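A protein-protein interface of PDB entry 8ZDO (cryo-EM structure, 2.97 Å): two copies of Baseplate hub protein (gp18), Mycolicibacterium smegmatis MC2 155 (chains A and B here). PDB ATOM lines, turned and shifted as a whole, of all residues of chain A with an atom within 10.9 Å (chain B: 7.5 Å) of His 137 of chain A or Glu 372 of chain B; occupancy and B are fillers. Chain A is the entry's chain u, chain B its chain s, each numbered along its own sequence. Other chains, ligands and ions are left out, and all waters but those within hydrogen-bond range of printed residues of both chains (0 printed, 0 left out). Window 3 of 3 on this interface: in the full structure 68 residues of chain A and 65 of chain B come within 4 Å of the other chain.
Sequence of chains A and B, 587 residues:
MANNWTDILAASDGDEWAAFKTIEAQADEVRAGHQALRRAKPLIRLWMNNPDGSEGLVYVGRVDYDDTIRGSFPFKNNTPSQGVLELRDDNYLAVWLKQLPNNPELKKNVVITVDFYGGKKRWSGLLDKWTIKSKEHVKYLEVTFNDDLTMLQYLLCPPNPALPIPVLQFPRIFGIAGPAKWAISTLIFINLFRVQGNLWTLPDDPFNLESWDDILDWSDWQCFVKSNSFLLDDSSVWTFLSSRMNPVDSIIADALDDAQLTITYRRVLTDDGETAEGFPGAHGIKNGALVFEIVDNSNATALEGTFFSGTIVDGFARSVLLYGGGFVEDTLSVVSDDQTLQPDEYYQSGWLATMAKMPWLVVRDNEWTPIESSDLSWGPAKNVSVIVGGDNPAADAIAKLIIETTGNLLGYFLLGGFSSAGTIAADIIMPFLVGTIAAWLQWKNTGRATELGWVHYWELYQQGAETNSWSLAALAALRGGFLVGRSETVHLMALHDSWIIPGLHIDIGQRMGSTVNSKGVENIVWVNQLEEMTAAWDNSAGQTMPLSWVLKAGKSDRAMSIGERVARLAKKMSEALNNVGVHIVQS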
ATOM      1  N   ASP A  89      25.970 -21.378  20.313  1.00  0.00           N
ATOM      2  CA  ASP A  89      26.519 -22.631  19.811  1.00  0.00           C
ATOM      3  C   ASP A  89      28.040 -22.664  19.856  1.00  0.00           C
ATOM      4  O   ASP A  89      28.624 -23.748  19.771  1.00  0.00           O
ATOM      5  CB  ASP A  89      26.028 -22.894  18.388  1.00  0.00           C
ATOM      6  CG  ASP A  89      24.783 -23.757  18.356  1.00  0.00           C
ATOM      7  OD1 ASP A  89      24.595 -24.568  19.286  1.00  0.00           O
ATOM      8  OD2 ASP A  89      23.989 -23.631  17.403  1.00  0.00           O
ATOM      9  N   ILE A 132      19.053 -27.461  18.547  1.00  0.00           N
ATOM     10  CA  ILE A 132      19.748 -26.399  17.832  1.00  0.00           C
ATOM     11  C   ILE A 132      18.688 -25.560  17.130  1.00  0.00           C
ATOM     12  O   ILE A 132      18.112 -25.986  16.128  1.00  0.00           O
ATOM     13  CB  ILE A 132      20.766 -26.962  16.835  1.00  0.00           C
ATOM     14  CG1 ILE A 132      21.718 -27.928  17.539  1.00  0.00           C
ATOM     15  CG2 ILE A 132      21.530 -25.838  16.165  1.00  0.00           C
ATOM     16  CD1 ILE A 132      22.722 -28.564  16.621  1.00  0.00           C
ATOM     17  N   LYS A 133      18.436 -24.366  17.650  1.00  0.00           N
ATOM     18  CA  LYS A 133      17.385 -23.493  17.153  1.00  0.00           C
ATOM     19  C   LYS A 133      17.994 -22.264  16.496  1.00  0.00           C
ATOM     20  O   LYS A 133      18.979 -21.708  16.986  1.00  0.00           O
ATOM     21  CB  LYS A 133      16.448 -23.073  18.285  1.00  0.00           C
ATOM     22  CG  LYS A 133      15.629 -24.213  18.849  1.00  0.00           C
ATOM     23  CD  LYS A 133      14.571 -23.708  19.806  1.00  0.00           C
ATOM     24  CE  LYS A 133      13.684 -24.841  20.284  1.00  0.00           C
ATOM     25  NZ  LYS A 133      12.690 -24.378  21.287  1.00  0.00           N
ATOM     26  N   SER A 134      17.394 -21.837  15.389  1.00  0.00           N
ATOM     27  CA  SER A 134      17.900 -20.727  14.597  1.00  0.00           C
ATOM     28  C   SER A 134      16.911 -19.573  14.624  1.00  0.00           C
ATOM     29  O   SER A 134      15.724 -19.757  14.337  1.00  0.00           O
ATOM     30  CB  SER A 134      18.154 -21.158  13.150  1.00  0.00           C
ATOM     31  OG  SER A 134      18.840 -22.395  13.096  1.00  0.00           O
ATOM     32  N   LYS A 135      17.404 -18.388  14.972  1.00  0.00           N
ATOM     33  CA  LYS A 135      16.682 -17.138  14.786  1.00  0.00           C
ATOM     34  C   LYS A 135      17.508 -16.251  13.865  1.00  0.00           C
ATOM     35  O   LYS A 135      18.656 -15.923  14.184  1.00  0.00           O
ATOM     36  CB  LYS A 135      16.409 -16.440  16.121  1.00  0.00           C
ATOM     37  CG  LYS A 135      17.603 -16.351  17.059  1.00  0.00           C
ATOM     38  CD  LYS A 135      17.221 -15.666  18.364  1.00  0.00           C
ATOM     39  CE  LYS A 135      18.442 -15.108  19.083  1.00  0.00           C
ATOM     40  NZ  LYS A 135      19.462 -16.154  19.378  1.00  0.00           N
ATOM     41  N   GLU A 136      16.920 -15.867  12.734  1.00  0.00           N
ATOM     42  CA  GLU A 136      17.565 -15.068  11.685  1.00  0.00           C
ATOM     43  C   GLU A 136      18.998 -15.538  11.419  1.00  0.00           C
ATOM     44  O   GLU A 136      19.971 -14.794  11.526  1.00  0.00           O
ATOM     45  CB  GLU A 136      17.470 -13.564  12.003  1.00  0.00           C
ATOM     46  CG  GLU A 136      18.078 -13.046  13.318  1.00  0.00           C
ATOM     47  CD  GLU A 136      19.504 -12.535  13.184  1.00  0.00           C
ATOM     48  OE1 GLU A 136      19.916 -12.191  12.056  1.00  0.00           O
ATOM     49  OE2 GLU A 136      20.211 -12.477  14.212  1.00  0.00           O
ATOM     50  N   HIS A 137      19.100 -16.816  11.050  1.00  0.00           N
ATOM     51  CA  HIS A 137      20.356 -17.460  10.662  1.00  0.00           C
ATOM     52  C   HIS A 137      21.363 -17.518  11.804  1.00  0.00           C
ATOM     53  O   HIS A 137      22.552 -17.756  11.574  1.00  0.00           O
ATOM     54  CB  HIS A 137      20.990 -16.775   9.446  1.00  0.00           C
ATOM     55  CG  HIS A 137      20.146 -16.832   8.212  1.00  0.00           C
ATOM     56  ND1 HIS A 137      19.459 -15.739   7.732  1.00  0.00           N
ATOM     57  CD2 HIS A 137      19.882 -17.848   7.357  1.00  0.00           C
ATOM     58  CE1 HIS A 137      18.805 -16.080   6.636  1.00  0.00           C
ATOM     59  NE2 HIS A 137      19.045 -17.354   6.388  1.00  0.00           N
ATOM     60  N   VAL A 138      20.912 -17.309  13.035  1.00  0.00           N
ATOM     61  CA  VAL A 138      21.766 -17.346  14.214  1.00  0.00           C
ATOM     62  C   VAL A 138      21.374 -18.572  15.021  1.00  0.00           C
ATOM     63  O   VAL A 138      20.213 -18.715  15.418  1.00  0.00           O
ATOM     64  CB  VAL A 138      21.629 -16.066  15.050  1.00  0.00           C
ATOM     65  CG1 VAL A 138      22.076 -16.312  16.475  1.00  0.00           C
ATOM     66  CG2 VAL A 138      22.430 -14.948  14.425  1.00  0.00           C
ATOM     67  N   LYS A 139      22.334 -19.453  15.269  1.00  0.00           N
ATOM     68  CA  LYS A 139      22.055 -20.742  15.883  1.00  0.00           C
ATOM     69  C   LYS A 139      22.459 -20.733  17.350  1.00  0.00           C
ATOM     70  O   LYS A 139      23.550 -20.272  17.699  1.00  0.00           O
ATOM     71  CB  LYS A 139      22.777 -21.863  15.135  1.00  0.00           C
ATOM     72  CG  LYS A 139      22.191 -22.138  13.764  1.00  0.00           C
ATOM     73  CD  LYS A 139      22.774 -23.385  13.138  1.00  0.00           C
ATOM     74  CE  LYS A 139      22.059 -23.713  11.839  1.00  0.00           C
ATOM     75  NZ  LYS A 139      22.764 -24.762  11.059  1.00  0.00           N
ATOM     76  N   TYR A 140      21.567 -21.230  18.200  1.00  0.00           N
ATOM     77  CA  TYR A 140      21.832 -21.401  19.617  1.00  0.00           C
ATOM     78  C   TYR A 140      21.332 -22.776  20.027  1.00  0.00           C
ATOM     79  O   TYR A 140      20.642 -23.461  19.272  1.00  0.00           O
ATOM     80  CB  TYR A 140      21.172 -20.300  20.456  1.00  0.00           C
ATOM     81  CG  TYR A 140      19.678 -20.190  20.272  1.00  0.00           C
ATOM     82  CD1 TYR A 140      19.143 -19.409  19.262  1.00  0.00           C
ATOM     83  CD2 TYR A 140      18.804 -20.860  21.114  1.00  0.00           C
ATOM     84  CE1 TYR A 140      17.782 -19.302  19.090  1.00  0.00           C
ATOM     85  CE2 TYR A 140      17.441 -20.761  20.949  1.00  0.00           C
ATOM     86  CZ  TYR A 140      16.934 -19.980  19.936  1.00  0.00           C
ATOM     87  OH  TYR A 140      15.574 -19.873  19.764  1.00  0.00           O
ATOM     88  N   VAL B 363      21.769 -34.124   3.199  1.00  0.00           N
ATOM     89  CA  VAL B 363      21.348 -32.739   3.055  1.00  0.00           C
ATOM     90  C   VAL B 363      22.274 -31.896   3.919  1.00  0.00           C
ATOM     91  O   VAL B 363      22.198 -31.933   5.152  1.00  0.00           O
ATOM     92  CB  VAL B 363      19.880 -32.559   3.458  1.00  0.00           C
ATOM     93  CG1 VAL B 363      19.497 -31.107   3.394  1.00  0.00           C
ATOM     94  CG2 VAL B 363      18.982 -33.401   2.571  1.00  0.00           C
ATOM     95  N   ASP B 365      24.176 -28.592   5.464  1.00  0.00           N
ATOM     96  CA  ASP B 365      23.932 -27.226   5.907  1.00  0.00           C
ATOM     97  C   ASP B 365      25.270 -26.549   6.176  1.00  0.00           C
ATOM     98  O   ASP B 365      26.087 -27.065   6.946  1.00  0.00           O
ATOM     99  CB  ASP B 365      23.052 -27.213   7.156  1.00  0.00           C
ATOM    100  CG  ASP B 365      22.901 -25.831   7.757  1.00  0.00           C
ATOM    101  OD1 ASP B 365      23.005 -24.835   7.013  1.00  0.00           O
ATOM    102  OD2 ASP B 365      22.677 -25.738   8.982  1.00  0.00           O
ATOM    103  N   ASN B 366      25.489 -25.407   5.539  1.00  0.00           N
ATOM    104  CA  ASN B 366      26.696 -24.613   5.730  1.00  0.00           C
ATOM    105  C   ASN B 366      26.326 -23.151   5.502  1.00  0.00           C
ATOM    106  O   ASN B 366      25.146 -22.787   5.533  1.00  0.00           O
ATOM    107  CB  ASN B 366      27.823 -25.104   4.806  1.00  0.00           C
ATOM    108  CG  ASN B 366      27.360 -25.312   3.382  1.00  0.00           C
ATOM    109  OD1 ASN B 366      26.165 -25.290   3.096  1.00  0.00           O
ATOM    110  ND2 ASN B 366      28.309 -25.511   2.477  1.00  0.00           N
ATOM    111  N   GLU B 367      27.335 -22.306   5.286  1.00  0.00           N
ATOM    112  CA  GLU B 367      27.069 -20.894   5.031  1.00  0.00           C
ATOM    113  C   GLU B 367      26.269 -20.697   3.752  1.00  0.00           C
ATOM    114  O   GLU B 367      25.459 -19.768   3.661  1.00  0.00           O
ATOM    115  CB  GLU B 367      28.382 -20.117   4.965  1.00  0.00           C
ATOM    116  CG  GLU B 367      28.217 -18.652   4.614  1.00  0.00           C
ATOM    117  CD  GLU B 367      29.524 -17.891   4.648  1.00  0.00           C
ATOM    118  OE1 GLU B 367      30.552 -18.488   5.027  1.00  0.00           O
ATOM    119  OE2 GLU B 367      29.523 -16.694   4.293  1.00  0.00           O
ATOM    120  N   THR B 369      24.085 -22.984   2.379  1.00  0.00           N
ATOM    121  CA  THR B 369      23.144 -24.086   2.298  1.00  0.00           C
ATOM    122  C   THR B 369      21.958 -23.708   1.412  1.00  0.00           C
ATOM    123  O   THR B 369      21.480 -22.571   1.460  1.00  0.00           O
ATOM    124  CB  THR B 369      22.655 -24.477   3.690  1.00  0.00           C
ATOM    125  OG1 THR B 369      21.633 -25.472   3.574  1.00  0.00           O
ATOM    126  CG2 THR B 369      22.101 -23.267   4.422  1.00  0.00           C
ATOM    127  N   PRO B 370      21.475 -24.631   0.576  1.00  0.00           N
ATOM    128  CA  PRO B 370      20.269 -24.355  -0.213  1.00  0.00           C
ATOM    129  C   PRO B 370      18.975 -24.578   0.546  1.00  0.00           C
ATOM    130  O   PRO B 370      17.907 -24.222   0.031  1.00  0.00           O
ATOM    131  CB  PRO B 370      20.395 -25.334  -1.382  1.00  0.00           C
ATOM    132  CG  PRO B 370      21.147 -26.484  -0.811  1.00  0.00           C
ATOM    133  CD  PRO B 370      22.080 -25.928   0.231  1.00  0.00           C
ATOM    134  N   ILE B 371      19.035 -25.148   1.749  1.00  0.00           N
ATOM    135  CA  ILE B 371      17.849 -25.417   2.552  1.00  0.00           C
ATOM    136  C   ILE B 371      17.843 -24.473   3.741  1.00  0.00           C
ATOM    137  O   ILE B 371      18.760 -23.662   3.909  1.00  0.00           O
ATOM    138  CB  ILE B 371      17.808 -26.873   3.041  1.00  0.00           C
ATOM    139  CG1 ILE B 371      18.868 -27.078   4.123  1.00  0.00           C
ATOM    140  CG2 ILE B 371      18.031 -27.829   1.888  1.00  0.00           C
ATOM    141  CD1 ILE B 371      18.582 -28.219   5.059  1.00  0.00           C
ATOM    142  N   GLU B 372      16.805 -24.562   4.567  1.00  0.00           N
ATOM    143  CA  GLU B 372      16.799 -23.931   5.881  1.00  0.00           C
ATOM    144  C   GLU B 372      16.580 -25.008   6.930  1.00  0.00           C
ATOM    145  O   GLU B 372      15.539 -25.669   6.935  1.00  0.00           O
ATOM    146  CB  GLU B 372      15.721 -22.852   5.982  1.00  0.00           C
ATOM    147  CG  GLU B 372      16.134 -21.508   5.405  1.00  0.00           C
ATOM    148  CD  GLU B 372      17.214 -20.827   6.223  1.00  0.00           C
ATOM    149  OE1 GLU B 372      17.231 -21.010   7.458  1.00  0.00           O
ATOM    150  OE2 GLU B 372      18.044 -20.107   5.631  1.00  0.00           O
ATOM    151  N   SER B 373      17.560 -25.188   7.811  1.00  0.00           N
ATOM    152  CA  SER B 373      17.430 -26.140   8.907  1.00  0.00           C
ATOM    153  C   SER B 373      16.706 -25.451  10.055  1.00  0.00           C
ATOM    154  O   SER B 373      17.239 -24.520  10.667  1.00  0.00           O
ATOM    155  CB  SER B 373      18.800 -26.648   9.341  1.00  0.00           C
ATOM    156  OG  SER B 373      19.526 -27.153   8.236  1.00  0.00           O
ATOM    157  N   SER B 374      15.482 -25.895  10.343  1.00  0.00           N
ATOM    158  CA  SER B 374      14.693 -25.261  11.391  1.00  0.00           C
ATOM    159  C   SER B 374      15.239 -25.608  12.769  1.00  0.00           C
ATOM    160  O   SER B 374      15.663 -24.725  13.522  1.00  0.00           O
ATOM    161  CB  SER B 374      13.228 -25.678  11.266  1.00  0.00           C
ATOM    162  OG  SER B 374      12.509 -25.370  12.446  1.00  0.00           O
ATOM    163  N   ASP B 375      15.241 -26.892  13.117  1.00  0.00           N
ATOM    164  CA  ASP B 375      15.762 -27.302  14.411  1.00  0.00           C
ATOM    165  C   ASP B 375      16.128 -28.779  14.378  1.00  0.00           C
ATOM    166  O   ASP B 375      15.416 -29.592  13.784  1.00  0.00           O
ATOM    167  CB  ASP B 375      14.757 -27.018  15.533  1.00  0.00           C
ATOM    168  CG  ASP B 375      13.375 -27.568  15.241  1.00  0.00           C
ATOM    169  OD1 ASP B 375      13.225 -28.803  15.149  1.00  0.00           O
ATOM    170  OD2 ASP B 375      12.433 -26.760  15.105  1.00  0.00           O
ATOM    171  N   HIS B 491      15.034 -33.931  13.045  1.00  0.00           N
ATOM    172  CA  HIS B 491      15.544 -32.783  12.313  1.00  0.00           C
ATOM    173  C   HIS B 491      14.453 -32.231  11.408  1.00  0.00           C
ATOM    174  O   HIS B 491      13.809 -32.987  10.673  1.00  0.00           O
ATOM    175  CB  HIS B 491      16.775 -33.167  11.490  1.00  0.00           C
ATOM    176  CG  HIS B 491      17.506 -31.998  10.911  1.00  0.00           C
ATOM    177  ND1 HIS B 491      18.624 -32.140  10.120  1.00  0.00           N
ATOM    178  CD2 HIS B 491      17.284 -30.667  11.011  1.00  0.00           C
ATOM    179  CE1 HIS B 491      19.058 -30.947   9.757  1.00  0.00           C
ATOM    180  NE2 HIS B 491      18.262 -30.036  10.284  1.00  0.00           N
ATOM    181  N   LEU B 492      14.252 -30.918  11.462  1.00  0.00           N
ATOM    182  CA  LEU B 492      13.314 -30.221  10.594  1.00  0.00           C
ATOM    183  C   LEU B 492      14.082 -29.476   9.514  1.00  0.00           C
ATOM    184  O   LEU B 492      14.976 -28.681   9.817  1.00  0.00           O
ATOM    185  CB  LEU B 492      12.448 -29.237  11.384  1.00  0.00           C
ATOM    186  CG  LEU B 492      11.195 -29.719  12.118  1.00  0.00           C
ATOM    187  CD1 LEU B 492      10.175 -30.242  11.121  1.00  0.00           C
ATOM    188  CD2 LEU B 492      11.509 -30.771  13.169  1.00  0.00           C
ATOM    189  N   MET B 493      13.721 -29.717   8.259  1.00  0.00           N
ATOM    190  CA  MET B 493      14.344 -29.061   7.123  1.00  0.00           C
ATOM    191  C   MET B 493      13.264 -28.422   6.267  1.00  0.00           C
ATOM    192  O   MET B 493      12.127 -28.890   6.226  1.00  0.00           O
ATOM    193  CB  MET B 493      15.158 -30.049   6.276  1.00  0.00           C
ATOM    194  CG  MET B 493      16.428 -30.540   6.936  1.00  0.00           C
ATOM    195  SD  MET B 493      16.757 -32.274   6.581  1.00  0.00           S
ATOM    196  CE  MET B 493      15.354 -33.050   7.373  1.00  0.00           C
ATOM    197  N   ALA B 494      13.627 -27.340   5.587  1.00  0.00           N
ATOM    198  CA  ALA B 494      12.741 -26.672   4.644  1.00  0.00           C
ATOM    199  C   ALA B 494      13.490 -26.549   3.328  1.00  0.00           C
ATOM    200  O   ALA B 494      14.491 -25.826   3.252  1.00  0.00           O
ATOM    201  CB  ALA B 494      12.310 -25.302   5.158  1.00  0.00           C
ATOM    202  N   LEU B 495      13.025 -27.265   2.305  1.00  0.00           N
ATOM    203  CA  LEU B 495      13.654 -27.227   0.992  1.00  0.00           C
ATOM    204  C   LEU B 495      13.016 -26.094   0.203  1.00  0.00           C
ATOM    205  O   LEU B 495      11.839 -26.168  -0.164  1.00  0.00           O
ATOM    206  CB  LEU B 495      13.496 -28.562   0.271  1.00  0.00           C
ATOM    207  CG  LEU B 495      13.613 -29.827   1.117  1.00  0.00           C
ATOM    208  CD1 LEU B 495      13.381 -31.047   0.264  1.00  0.00           C
ATOM    209  CD2 LEU B 495      14.972 -29.899   1.778  1.00  0.00           C
ATOM    210  N   HIS B 496      13.788 -25.042  -0.054  1.00  0.00           N
ATOM    211  CA  HIS B 496      13.245 -23.850  -0.689  1.00  0.00           C
ATOM    212  C   HIS B 496      13.409 -23.898  -2.204  1.00  0.00           C
ATOM    213  O   HIS B 496      12.421 -23.905  -2.945  1.00  0.00           O
ATOM    214  CB  HIS B 496      13.924 -22.610  -0.103  1.00  0.00           C
ATOM    215  CG  HIS B 496      13.599 -22.372   1.337  1.00  0.00           C
ATOM    216  ND1 HIS B 496      12.371 -21.902   1.751  1.00  0.00           N
ATOM    217  CD2 HIS B 496      14.338 -22.536   2.457  1.00  0.00           C
ATOM    218  CE1 HIS B 496      12.369 -21.789   3.068  1.00  0.00           C
ATOM    219  NE2 HIS B 496      13.550 -22.168   3.519  1.00  0.00           N
ATOM    220  N   SER B 498      16.249 -26.034  -3.251  1.00  0.00           N
ATOM    221  CA  SER B 498      17.250 -27.081  -3.333  1.00  0.00           C
ATOM    222  C   SER B 498      16.891 -28.068  -4.433  1.00  0.00           C
ATOM    223  O   SER B 498      15.725 -28.242  -4.788  1.00  0.00           O
ATOM    224  CB  SER B 498      17.366 -27.805  -1.994  1.00  0.00           C
ATOM    225  OG  SER B 498      18.217 -28.930  -2.099  1.00  0.00           O
ATOM    226  N   ASN B 517      24.957 -26.793  10.643  1.00  0.00           N
ATOM    227  CA  ASN B 517      26.178 -25.988  10.652  1.00  0.00           C
ATOM    228  C   ASN B 517      26.369 -25.370  12.037  1.00  0.00           C
ATOM    229  O   ASN B 517      26.242 -24.163  12.249  1.00  0.00           O
ATOM    230  CB  ASN B 517      26.128 -24.923   9.566  1.00  0.00           C
ATOM    231  CG  ASN B 517      27.506 -24.449   9.152  1.00  0.00           C
ATOM    232  OD1 ASN B 517      28.401 -25.254   8.895  1.00  0.00           O
ATOM    233  ND2 ASN B 517      27.685 -23.136   9.086  1.00  0.00           N
ATOM    234  N   VAL B 550       8.509 -29.129   3.186  1.00  0.00           N
ATOM    235  CA  VAL B 550       9.117 -29.144   4.509  1.00  0.00           C
ATOM    236  C   VAL B 550       9.243 -30.594   4.944  1.00  0.00           C
ATOM    237  O   VAL B 550       8.244 -31.318   4.999  1.00  0.00           O
ATOM    238  CB  VAL B 550       8.295 -28.335   5.523  1.00  0.00           C
ATOM    239  CG1 VAL B 550       8.791 -28.599   6.927  1.00  0.00           C
ATOM    240  CG2 VAL B 550       8.366 -26.856   5.199  1.00  0.00           C
ATOM    241  N   LEU B 551      10.465 -31.015   5.253  1.00  0.00           N
ATOM    242  CA  LEU B 551      10.747 -32.371   5.690  1.00  0.00           C
ATOM    243  C   LEU B 551      10.957 -32.416   7.198  1.00  0.00           C
ATOM    244  O   LEU B 551      11.479 -31.478   7.803  1.00  0.00           O
ATOM    245  CB  LEU B 551      11.992 -32.928   4.999  1.00  0.00           C
ATOM    246  CG  LEU B 551      12.171 -32.767   3.491  1.00  0.00           C
ATOM    247  CD1 LEU B 551      13.474 -33.413   3.063  1.00  0.00           C
ATOM    248  CD2 LEU B 551      11.009 -33.371   2.734  1.00  0.00           C
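A ring nitrogen (NE2) of His 137 of chain A sits at hydrogen-bond distance from the side-chain carboxylate (OE2) of Glu 372 of chain B (3.0 Å).
N of Asn 517 of chain B lies close to NZ of Lys 139 of chain A (3.0 Å).
NZ of Lys 139 of chain A sits close to OD2 of Asp 365 of chain B (2.3 Å).
N of Ala 494 of chain B is in hydrogen-bond range of O of Glu 372 of chain B (2.9 Å).
The side-chain carboxylate of Asp 365 of chain B is in hydrogen-bond range of the backbone NH of Asn 517 of chain B (3.0 Å).
The backbone NH (N) of Leu 492 of chain B sits at hydrogen-bond distance from the backbone carbonyl oxygen (O) of Asp 375 of chain B.
OG of Ser 374 of chain B is in hydrogen-bond range of OD2 of Asp 375 of chain B (3.0 Å).
The backbone carbonyl oxygen (O) of Leu 492 of chain B sits at hydrogen-bond distance from the backbone NH (N) of Ser 374 of chain B (2.9 Å).
Among the printed residues, pairs that only touch across the chains: Ile 132 of chain A with Asp 375 of chain B (3.2 Å), Ser 134 of chain A with Ser 373 of chain B (3.6 Å), Ile 132 of chain A with Ser 374 of chain B (3.8 Å) and Ser 134 of chain A with Ser 374 of chain B (3.9 Å).
Of the printed residues of chain B, Ile 132 of chain A touches Ser 374 (3.8 Å) and Asp 375 (3.2 Å).
Printed residues of chain B within 4 Å of Ser 134 of chain A: Ser 373 (3.6 Å) and Ser 374 (3.9 Å).
Of chain B, only Glu 372 comes within 4 Å of His 137 of chain A.
Of the printed residues of chain B, Lys 139 of chain A touches Asp 365 (2.3 Å) and Asn 517 (3.0 Å).
Of the printed residues of chain A, Asp 365 of chain B touches Lys 139.
No residue of chain A comes within 4 Å of Ile 371 of chain B.
Of chain A, only His 137 (3.0 Å) comes within 4 Å of Glu 372 of chain B.
Printed residues of chain A within 4 Å of Ser 373 of chain B: Ser 134.
No residue of chain A comes within 4 Å of Ala 494 of chain B.
Val 550 of chain B touches none of the printed residues of chain A.
The nearest residue of chain A that does not touch Glu 372 of chain B is Ser 134 of chain A (5.8 Å).
Hydrophobic or aromatic side chains of chain A that line the printed part of chain B: His 137.
No position is printed for both chains.
Of the 7 pairs that touch across the chains among the printed residues, none has its exchanged pair printed and touching as well.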
